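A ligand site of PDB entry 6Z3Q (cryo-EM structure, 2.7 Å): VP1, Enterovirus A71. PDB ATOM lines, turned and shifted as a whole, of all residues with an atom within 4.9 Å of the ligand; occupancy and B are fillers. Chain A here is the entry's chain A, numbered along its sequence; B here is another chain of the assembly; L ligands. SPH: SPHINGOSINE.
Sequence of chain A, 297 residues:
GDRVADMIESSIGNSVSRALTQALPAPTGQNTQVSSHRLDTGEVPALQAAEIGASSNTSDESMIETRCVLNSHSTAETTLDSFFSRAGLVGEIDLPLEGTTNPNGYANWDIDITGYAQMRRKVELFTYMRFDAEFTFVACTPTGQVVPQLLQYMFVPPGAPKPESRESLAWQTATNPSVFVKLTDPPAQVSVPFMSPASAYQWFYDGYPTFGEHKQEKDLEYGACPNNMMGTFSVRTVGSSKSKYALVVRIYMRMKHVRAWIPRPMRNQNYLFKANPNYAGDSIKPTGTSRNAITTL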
ATOM      1  N   ILE A 111      16.833  15.422  29.880  1.00  0.00           N
ATOM      2  CA  ILE A 111      17.367  16.672  29.362  1.00  0.00           C
ATOM      3  C   ILE A 111      16.217  17.600  29.013  1.00  0.00           C
ATOM      4  O   ILE A 111      15.269  17.211  28.323  1.00  0.00           O
ATOM      5  CB  ILE A 111      18.259  16.404  28.140  1.00  0.00           C
ATOM      6  CG1 ILE A 111      19.345  15.384  28.506  1.00  0.00           C
ATOM      7  CG2 ILE A 111      18.901  17.702  27.664  1.00  0.00           C
ATOM      8  CD1 ILE A 111      20.134  14.885  27.321  1.00  0.00           C
ATOM      9  N   ASP A 112      16.298  18.835  29.508  1.00  0.00           N
ATOM     10  CA  ASP A 112      15.291  19.846  29.220  1.00  0.00           C
ATOM     11  C   ASP A 112      15.807  21.199  29.684  1.00  0.00           C
ATOM     12  O   ASP A 112      16.374  21.311  30.774  1.00  0.00           O
ATOM     13  CB  ASP A 112      13.959  19.512  29.883  1.00  0.00           C
ATOM     14  CG  ASP A 112      14.118  19.148  31.338  1.00  0.00           C
ATOM     15  OD1 ASP A 112      15.248  19.267  31.866  1.00  0.00           O
ATOM     16  OD2 ASP A 112      13.117  18.731  31.963  1.00  0.00           O
ATOM     17  N   ILE A 113      15.597  22.217  28.855  1.00  0.00           N
ATOM     18  CA  ILE A 113      16.067  23.557  29.177  1.00  0.00           C
ATOM     19  C   ILE A 113      15.114  24.292  30.110  1.00  0.00           C
ATOM     20  O   ILE A 113      15.499  25.334  30.664  1.00  0.00           O
ATOM     21  CB  ILE A 113      16.263  24.379  27.884  1.00  0.00           C
ATOM     22  CG1 ILE A 113      17.153  23.619  26.901  1.00  0.00           C
ATOM     23  CG2 ILE A 113      16.834  25.746  28.194  1.00  0.00           C
ATOM     24  CD1 ILE A 113      18.509  23.262  27.456  1.00  0.00           C
ATOM     25  N   THR A 114      13.908  23.778  30.323  1.00  0.00           N
ATOM     26  CA  THR A 114      12.843  24.511  30.991  1.00  0.00           C
ATOM     27  C   THR A 114      12.828  24.305  32.500  1.00  0.00           C
ATOM     28  O   THR A 114      11.757  24.418  33.116  1.00  0.00           O
ATOM     29  CB  THR A 114      11.499  24.117  30.387  1.00  0.00           C
ATOM     30  OG1 THR A 114      11.355  22.702  30.427  1.00  0.00           O
ATOM     31  CG2 THR A 114      11.402  24.587  28.946  1.00  0.00           C
ATOM     32  N   PHE A 131      19.779  24.378  16.911  1.00  0.00           N
ATOM     33  CA  PHE A 131      21.091  24.817  17.368  1.00  0.00           C
ATOM     34  C   PHE A 131      21.926  23.605  17.770  1.00  0.00           C
ATOM     35  O   PHE A 131      21.398  22.523  18.045  1.00  0.00           O
ATOM     36  CB  PHE A 131      20.959  25.786  18.539  1.00  0.00           C
ATOM     37  CG  PHE A 131      20.173  25.244  19.699  1.00  0.00           C
ATOM     38  CD1 PHE A 131      18.841  25.571  19.859  1.00  0.00           C
ATOM     39  CD2 PHE A 131      20.767  24.400  20.627  1.00  0.00           C
ATOM     40  CE1 PHE A 131      18.126  25.076  20.920  1.00  0.00           C
ATOM     41  CE2 PHE A 131      20.052  23.905  21.688  1.00  0.00           C
ATOM     42  CZ  PHE A 131      18.725  24.238  21.827  1.00  0.00           C
ATOM     43  N   ALA A 133      24.510  22.398  20.726  1.00  0.00           N
ATOM     44  CA  ALA A 133      24.726  22.750  22.125  1.00  0.00           C
ATOM     45  C   ALA A 133      26.196  22.552  22.497  1.00  0.00           C
ATOM     46  O   ALA A 133      26.919  21.769  21.886  1.00  0.00           O
ATOM     47  CB  ALA A 133      23.840  21.912  23.035  1.00  0.00           C
ATOM     48  N   PHE A 135      27.773  21.765  26.224  1.00  0.00           N
ATOM     49  CA  PHE A 135      27.446  21.471  27.606  1.00  0.00           C
ATOM     50  C   PHE A 135      28.702  21.427  28.453  1.00  0.00           C
ATOM     51  O   PHE A 135      29.693  20.783  28.076  1.00  0.00           O
ATOM     52  CB  PHE A 135      26.701  20.143  27.717  1.00  0.00           C
ATOM     53  CG  PHE A 135      25.246  20.244  27.469  1.00  0.00           C
ATOM     54  CD1 PHE A 135      24.363  20.383  28.522  1.00  0.00           C
ATOM     55  CD2 PHE A 135      24.737  20.219  26.188  1.00  0.00           C
ATOM     56  CE1 PHE A 135      23.016  20.494  28.302  1.00  0.00           C
ATOM     57  CE2 PHE A 135      23.383  20.329  25.962  1.00  0.00           C
ATOM     58  CZ  PHE A 135      22.523  20.462  27.018  1.00  0.00           C
ATOM     59  N   PHE A 137      30.067  20.793  32.517  1.00  0.00           N
ATOM     60  CA  PHE A 137      29.723  20.155  33.770  1.00  0.00           C
ATOM     61  C   PHE A 137      30.697  20.628  34.835  1.00  0.00           C
ATOM     62  O   PHE A 137      31.919  20.510  34.652  1.00  0.00           O
ATOM     63  CB  PHE A 137      29.765  18.631  33.636  1.00  0.00           C
ATOM     64  CG  PHE A 137      29.054  18.127  32.411  1.00  0.00           C
ATOM     65  CD1 PHE A 137      27.680  17.998  32.402  1.00  0.00           C
ATOM     66  CD2 PHE A 137      29.760  17.799  31.267  1.00  0.00           C
ATOM     67  CE1 PHE A 137      27.027  17.546  31.291  1.00  0.00           C
ATOM     68  CE2 PHE A 137      29.100  17.347  30.149  1.00  0.00           C
ATOM     69  CZ  PHE A 137      27.734  17.215  30.160  1.00  0.00           C
ATOM     70  N   TYR A 153      29.933  10.513  33.399  1.00  0.00           N
ATOM     71  CA  TYR A 153      28.748  11.082  32.776  1.00  0.00           C
ATOM     72  C   TYR A 153      28.455  10.262  31.519  1.00  0.00           C
ATOM     73  O   TYR A 153      29.313  10.165  30.643  1.00  0.00           O
ATOM     74  CB  TYR A 153      28.948  12.539  32.399  1.00  0.00           C
ATOM     75  CG  TYR A 153      29.417  13.451  33.513  1.00  0.00           C
ATOM     76  CD1 TYR A 153      28.844  13.398  34.768  1.00  0.00           C
ATOM     77  CD2 TYR A 153      30.413  14.379  33.289  1.00  0.00           C
ATOM     78  CE1 TYR A 153      29.265  14.248  35.774  1.00  0.00           C
ATOM     79  CE2 TYR A 153      30.843  15.223  34.285  1.00  0.00           C
ATOM     80  CZ  TYR A 153      30.267  15.151  35.530  1.00  0.00           C
ATOM     81  OH  TYR A 153      30.703  15.997  36.519  1.00  0.00           O
ATOM     82  N   MET A 154      27.268   9.702  31.425  1.00  0.00           N
ATOM     83  CA  MET A 154      26.842   8.960  30.253  1.00  0.00           C
ATOM     84  C   MET A 154      25.598   9.602  29.663  1.00  0.00           C
ATOM     85  O   MET A 154      24.640   9.901  30.369  1.00  0.00           O
ATOM     86  CB  MET A 154      26.572   7.492  30.605  1.00  0.00           C
ATOM     87  CG  MET A 154      26.295   6.611  29.407  1.00  0.00           C
ATOM     88  SD  MET A 154      26.278   4.857  29.805  1.00  0.00           S
ATOM     89  CE  MET A 154      25.097   4.803  31.143  1.00  0.00           C
ATOM     90  N   PHE A 155      25.626   9.823  28.351  1.00  0.00           N
ATOM     91  CA  PHE A 155      24.456  10.312  27.624  1.00  0.00           C
ATOM     92  C   PHE A 155      23.714   9.099  27.092  1.00  0.00           C
ATOM     93  O   PHE A 155      24.239   8.372  26.249  1.00  0.00           O
ATOM     94  CB  PHE A 155      24.856  11.253  26.488  1.00  0.00           C
ATOM     95  CG  PHE A 155      23.751  11.525  25.519  1.00  0.00           C
ATOM     96  CD1 PHE A 155      22.531  12.010  25.952  1.00  0.00           C
ATOM     97  CD2 PHE A 155      23.928  11.297  24.166  1.00  0.00           C
ATOM     98  CE1 PHE A 155      21.514  12.257  25.050  1.00  0.00           C
ATOM     99  CE2 PHE A 155      22.905  11.541  23.272  1.00  0.00           C
ATOM    100  CZ  PHE A 155      21.701  12.027  23.718  1.00  0.00           C
ATOM    101  N   PRO A 177      27.827   7.525  24.378  1.00  0.00           N
ATOM    102  CA  PRO A 177      28.872   8.504  24.716  1.00  0.00           C
ATOM    103  C   PRO A 177      29.018   8.629  26.222  1.00  0.00           C
ATOM    104  O   PRO A 177      28.030   8.662  26.961  1.00  0.00           O
ATOM    105  CB  PRO A 177      28.355   9.806  24.085  1.00  0.00           C
ATOM    106  CG  PRO A 177      27.385   9.388  23.060  1.00  0.00           C
ATOM    107  CD  PRO A 177      26.763   8.133  23.556  1.00  0.00           C
ATOM    108  N   SER A 178      30.264   8.738  26.680  1.00  0.00           N
ATOM    109  CA  SER A 178      30.557   8.864  28.094  1.00  0.00           C
ATOM    110  C   SER A 178      31.794   9.717  28.297  1.00  0.00           C
ATOM    111  O   SER A 178      32.602   9.918  27.389  1.00  0.00           O
ATOM    112  CB  SER A 178      30.745   7.482  28.740  1.00  0.00           C
ATOM    113  OG  SER A 178      31.039   7.597  30.108  1.00  0.00           O
ATOM    114  N   VAL A 179      31.920  10.232  29.518  1.00  0.00           N
ATOM    115  CA  VAL A 179      33.019  11.118  29.906  1.00  0.00           C
ATOM    116  C   VAL A 179      33.419  10.775  31.329  1.00  0.00           C
ATOM    117  O   VAL A 179      32.578  10.776  32.236  1.00  0.00           O
ATOM    118  CB  VAL A 179      32.621  12.597  29.811  1.00  0.00           C
ATOM    119  CG1 VAL A 179      33.655  13.471  30.484  1.00  0.00           C
ATOM    120  CG2 VAL A 179      32.457  13.012  28.359  1.00  0.00           C
ATOM    121  N   VAL A 190      31.708  19.434  26.410  1.00  0.00           N
ATOM    122  CA  VAL A 190      31.472  18.682  25.190  1.00  0.00           C
ATOM    123  C   VAL A 190      30.528  19.476  24.313  1.00  0.00           C
ATOM    124  O   VAL A 190      29.857  20.409  24.767  1.00  0.00           O
ATOM    125  CB  VAL A 190      30.879  17.270  25.466  1.00  0.00           C
ATOM    126  CG1 VAL A 190      31.786  16.488  26.399  1.00  0.00           C
ATOM    127  CG2 VAL A 190      29.485  17.388  26.054  1.00  0.00           C
ATOM    128  N   VAL A 192      27.319  18.968  21.549  1.00  0.00           N
ATOM    129  CA  VAL A 192      26.253  18.062  21.140  1.00  0.00           C
ATOM    130  C   VAL A 192      25.660  18.595  19.849  1.00  0.00           C
ATOM    131  O   VAL A 192      25.456  19.809  19.730  1.00  0.00           O
ATOM    132  CB  VAL A 192      25.164  17.946  22.227  1.00  0.00           C
ATOM    133  CG1 VAL A 192      24.128  16.918  21.836  1.00  0.00           C
ATOM    134  CG2 VAL A 192      25.791  17.612  23.560  1.00  0.00           C
ATOM    135  N   PRO A 193      25.363  17.747  18.869  1.00  0.00           N
ATOM    136  CA  PRO A 193      24.745  18.212  17.626  1.00  0.00           C
ATOM    137  C   PRO A 193      23.250  18.434  17.810  1.00  0.00           C
ATOM    138  O   PRO A 193      22.693  18.315  18.899  1.00  0.00           O
ATOM    139  CB  PRO A 193      25.023  17.065  16.660  1.00  0.00           C
ATOM    140  CG  PRO A 193      25.057  15.876  17.515  1.00  0.00           C
ATOM    141  CD  PRO A 193      25.610  16.300  18.847  1.00  0.00           C
ATOM    142  N   MET A 195      19.931  16.919  17.458  1.00  0.00           N
ATOM    143  CA  MET A 195      19.559  15.509  17.469  1.00  0.00           C
ATOM    144  C   MET A 195      18.058  15.284  17.381  1.00  0.00           C
ATOM    145  O   MET A 195      17.597  14.164  17.614  1.00  0.00           O
ATOM    146  CB  MET A 195      20.117  14.842  18.716  1.00  0.00           C
ATOM    147  CG  MET A 195      21.622  15.000  18.878  1.00  0.00           C
ATOM    148  SD  MET A 195      22.292  14.076  20.268  1.00  0.00           S
ATOM    149  CE  MET A 195      21.381  14.808  21.609  1.00  0.00           C
ATOM    150  N   TYR A 201      13.903  22.142  17.360  1.00  0.00           N
ATOM    151  CA  TYR A 201      13.214  21.997  18.630  1.00  0.00           C
ATOM    152  C   TYR A 201      12.093  23.008  18.713  1.00  0.00           C
ATOM    153  O   TYR A 201      12.199  24.133  18.217  1.00  0.00           O
ATOM    154  CB  TYR A 201      14.168  22.211  19.806  1.00  0.00           C
ATOM    155  CG  TYR A 201      15.413  21.363  19.786  1.00  0.00           C
ATOM    156  CD1 TYR A 201      15.322  19.979  19.885  1.00  0.00           C
ATOM    157  CD2 TYR A 201      16.669  21.936  19.695  1.00  0.00           C
ATOM    158  CE1 TYR A 201      16.456  19.205  19.882  1.00  0.00           C
ATOM    159  CE2 TYR A 201      17.802  21.162  19.692  1.00  0.00           C
ATOM    160  CZ  TYR A 201      17.692  19.797  19.782  1.00  0.00           C
ATOM    161  OH  TYR A 201      18.828  19.014  19.777  1.00  0.00           O
ATOM    162  N   TRP A 203       9.578  24.676  21.698  1.00  0.00           N
ATOM    163  CA  TRP A 203       9.257  24.784  23.114  1.00  0.00           C
ATOM    164  C   TRP A 203       7.756  24.771  23.361  1.00  0.00           C
ATOM    165  O   TRP A 203       7.343  24.641  24.515  1.00  0.00           O
ATOM    166  CB  TRP A 203       9.863  26.058  23.706  1.00  0.00           C
ATOM    167  CG  TRP A 203      11.157  26.438  23.084  1.00  0.00           C
ATOM    168  CD1 TRP A 203      11.372  27.472  22.242  1.00  0.00           C
ATOM    169  CD2 TRP A 203      12.416  25.776  23.235  1.00  0.00           C
ATOM    170  NE1 TRP A 203      12.688  27.503  21.856  1.00  0.00           N
ATOM    171  CE2 TRP A 203      13.350  26.471  22.460  1.00  0.00           C
ATOM    172  CE3 TRP A 203      12.842  24.653  23.959  1.00  0.00           C
ATOM    173  CZ2 TRP A 203      14.689  26.096  22.384  1.00  0.00           C
ATOM    174  CZ3 TRP A 203      14.166  24.285  23.886  1.00  0.00           C
ATOM    175  CH2 TRP A 203      15.078  25.008  23.103  1.00  0.00           C
ATOM    176  N   ASN A 228      11.404  16.675  21.241  1.00  0.00           N
ATOM    177  CA  ASN A 228      12.221  17.411  22.182  1.00  0.00           C
ATOM    178  C   ASN A 228      12.915  16.530  23.195  1.00  0.00           C
ATOM    179  O   ASN A 228      13.860  16.988  23.855  1.00  0.00           O
ATOM    180  CB  ASN A 228      11.365  18.437  22.931  1.00  0.00           C
ATOM    181  CG  ASN A 228      10.952  19.596  22.054  1.00  0.00           C
ATOM    182  OD1 ASN A 228      11.648  19.949  21.098  1.00  0.00           O
ATOM    183  ND2 ASN A 228       9.827  20.210  22.373  1.00  0.00           N
ATOM    184  N   MET A 230      15.478  14.248  24.070  1.00  0.00           N
ATOM    185  CA  MET A 230      16.746  13.837  23.488  1.00  0.00           C
ATOM    186  C   MET A 230      17.506  12.838  24.343  1.00  0.00           C
ATOM    187  O   MET A 230      18.688  12.600  24.090  1.00  0.00           O
ATOM    188  CB  MET A 230      17.625  15.063  23.216  1.00  0.00           C
ATOM    189  CG  MET A 230      17.082  16.001  22.150  1.00  0.00           C
ATOM    190  SD  MET A 230      16.930  15.219  20.519  1.00  0.00           S
ATOM    191  CE  MET A 230      15.257  14.589  20.571  1.00  0.00           C
ATOM    192  N   PHE A 233      20.772  12.212  30.954  1.00  0.00           N
ATOM    193  CA  PHE A 233      22.157  12.372  31.373  1.00  0.00           C
ATOM    194  C   PHE A 233      22.295  11.652  32.705  1.00  0.00           C
ATOM    195  O   PHE A 233      21.667  12.051  33.697  1.00  0.00           O
ATOM    196  CB  PHE A 233      22.503  13.853  31.493  1.00  0.00           C
ATOM    197  CG  PHE A 233      23.791  14.132  32.182  1.00  0.00           C
ATOM    198  CD1 PHE A 233      24.936  14.354  31.450  1.00  0.00           C
ATOM    199  CD2 PHE A 233      23.862  14.182  33.565  1.00  0.00           C
ATOM    200  CE1 PHE A 233      26.115  14.621  32.081  1.00  0.00           C
ATOM    201  CE2 PHE A 233      25.051  14.439  34.201  1.00  0.00           C
ATOM    202  CZ  PHE A 233      26.181  14.660  33.455  1.00  0.00           C
ATOM    203  N   MET A 253      24.742  25.148  29.553  1.00  0.00           N
ATOM    204  CA  MET A 253      24.632  24.922  28.118  1.00  0.00           C
ATOM    205  C   MET A 253      24.671  26.257  27.400  1.00  0.00           C
ATOM    206  O   MET A 253      23.967  27.193  27.800  1.00  0.00           O
ATOM    207  CB  MET A 253      23.339  24.181  27.775  1.00  0.00           C
ATOM    208  CG  MET A 253      23.209  23.821  26.309  1.00  0.00           C
ATOM    209  SD  MET A 253      21.518  23.411  25.841  1.00  0.00           S
ATOM    210  CE  MET A 253      20.754  25.025  25.942  1.00  0.00           C
ATOM    211  N   ILE B  24      30.505  14.662  20.827  1.00  0.00           N
ATOM    212  CA  ILE B  24      30.186  13.384  21.465  1.00  0.00           C
ATOM    213  C   ILE B  24      29.749  12.331  20.459  1.00  0.00           C
ATOM    214  O   ILE B  24      29.883  11.131  20.732  1.00  0.00           O
ATOM    215  CB  ILE B  24      29.082  13.564  22.523  1.00  0.00           C
ATOM    216  CG1 ILE B  24      27.828  14.187  21.916  1.00  0.00           C
ATOM    217  CG2 ILE B  24      29.579  14.426  23.654  1.00  0.00           C
ATOM    218  CD1 ILE B  24      26.587  13.926  22.730  1.00  0.00           C
HETATM  219  C1  SPH L   1      12.854  20.398  26.010  1.00  0.00           C
HETATM  220  O1  SPH L   1      12.643  21.587  26.746  1.00  0.00           O
HETATM  221  C2  SPH L   1      14.299  20.269  25.531  1.00  0.00           C
HETATM  222  N2  SPH L   1      14.823  18.979  25.910  1.00  0.00           N
HETATM  223  C3  SPH L   1      14.371  20.387  24.007  1.00  0.00           C
HETATM  224  O3  SPH L   1      13.707  21.549  23.580  1.00  0.00           O
HETATM  225  C4  SPH L   1      15.794  20.378  23.531  1.00  0.00           C
HETATM  226  C5  SPH L   1      16.801  21.261  24.129  1.00  0.00           C
HETATM  227  C6  SPH L   1      18.246  21.113  23.740  1.00  0.00           C
HETATM  228  C7  SPH L   1      18.717  19.664  23.826  1.00  0.00           C
HETATM  229  C8  SPH L   1      20.200  19.585  23.498  1.00  0.00           C
HETATM  230  C9  SPH L   1      20.615  18.179  23.070  1.00  0.00           C
HETATM  231  C10 SPH L   1      20.491  17.149  24.186  1.00  0.00           C
HETATM  232  C11 SPH L   1      21.574  17.348  25.232  1.00  0.00           C
HETATM  233  C12 SPH L   1      22.515  16.151  25.332  1.00  0.00           C
HETATM  234  C13 SPH L   1      23.427  16.275  26.545  1.00  0.00           C
HETATM  235  C14 SPH L   1      24.397  15.099  26.582  1.00  0.00           C
HETATM  236  C15 SPH L   1      25.563  15.358  27.531  1.00  0.00           C
HETATM  237  C16 SPH L   1      26.775  14.545  27.108  1.00  0.00           C
HETATM  238  C17 SPH L   1      27.447  13.880  28.316  1.00  0.00           C
HETATM  239  C18 SPH L   1      28.630  13.033  27.868  1.00  0.00           C
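Residues that only touch the ligand: Trp 203, Asp 112, Phe 135, Met 195, Ile 113, Phe 155, Met 230, Phe 131, Tyr 201, Phe 137, Val 179, Thr 114 and Val 192.
The nearest printed residue that does not touch the ligand is Phe 233 (4.04 Å).
The backbone carbonyl oxygen of Asn 228 lies within hydrogen-bond range of a nitrogen (N2) of the ligand (3.0 Å).
A nitrogen (N2) of the ligand sits at hydrogen-bond distance from the backbone carbonyl oxygen (O) of Ile 111 (3.0 Å).
N of Phe 135 is in hydrogen-bond range of O of Val 190 (2.9 Å).
The backbone NH of Met 195 is in hydrogen-bond range of the side-chain hydroxyl of Tyr 201.
The backbone carbonyl oxygen of Pro 177 is in hydrogen-bond range of the backbone NH of Phe 155, 3.0 Å away.
The backbone carbonyl oxygen of Tyr 153 lies within hydrogen-bond range of the backbone NH of Val 179 (2.8 Å).
The backbone NH (N) of Val 192 lies within hydrogen-bond range of the backbone carbonyl oxygen (O) of Ala 133 (2.8 Å).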
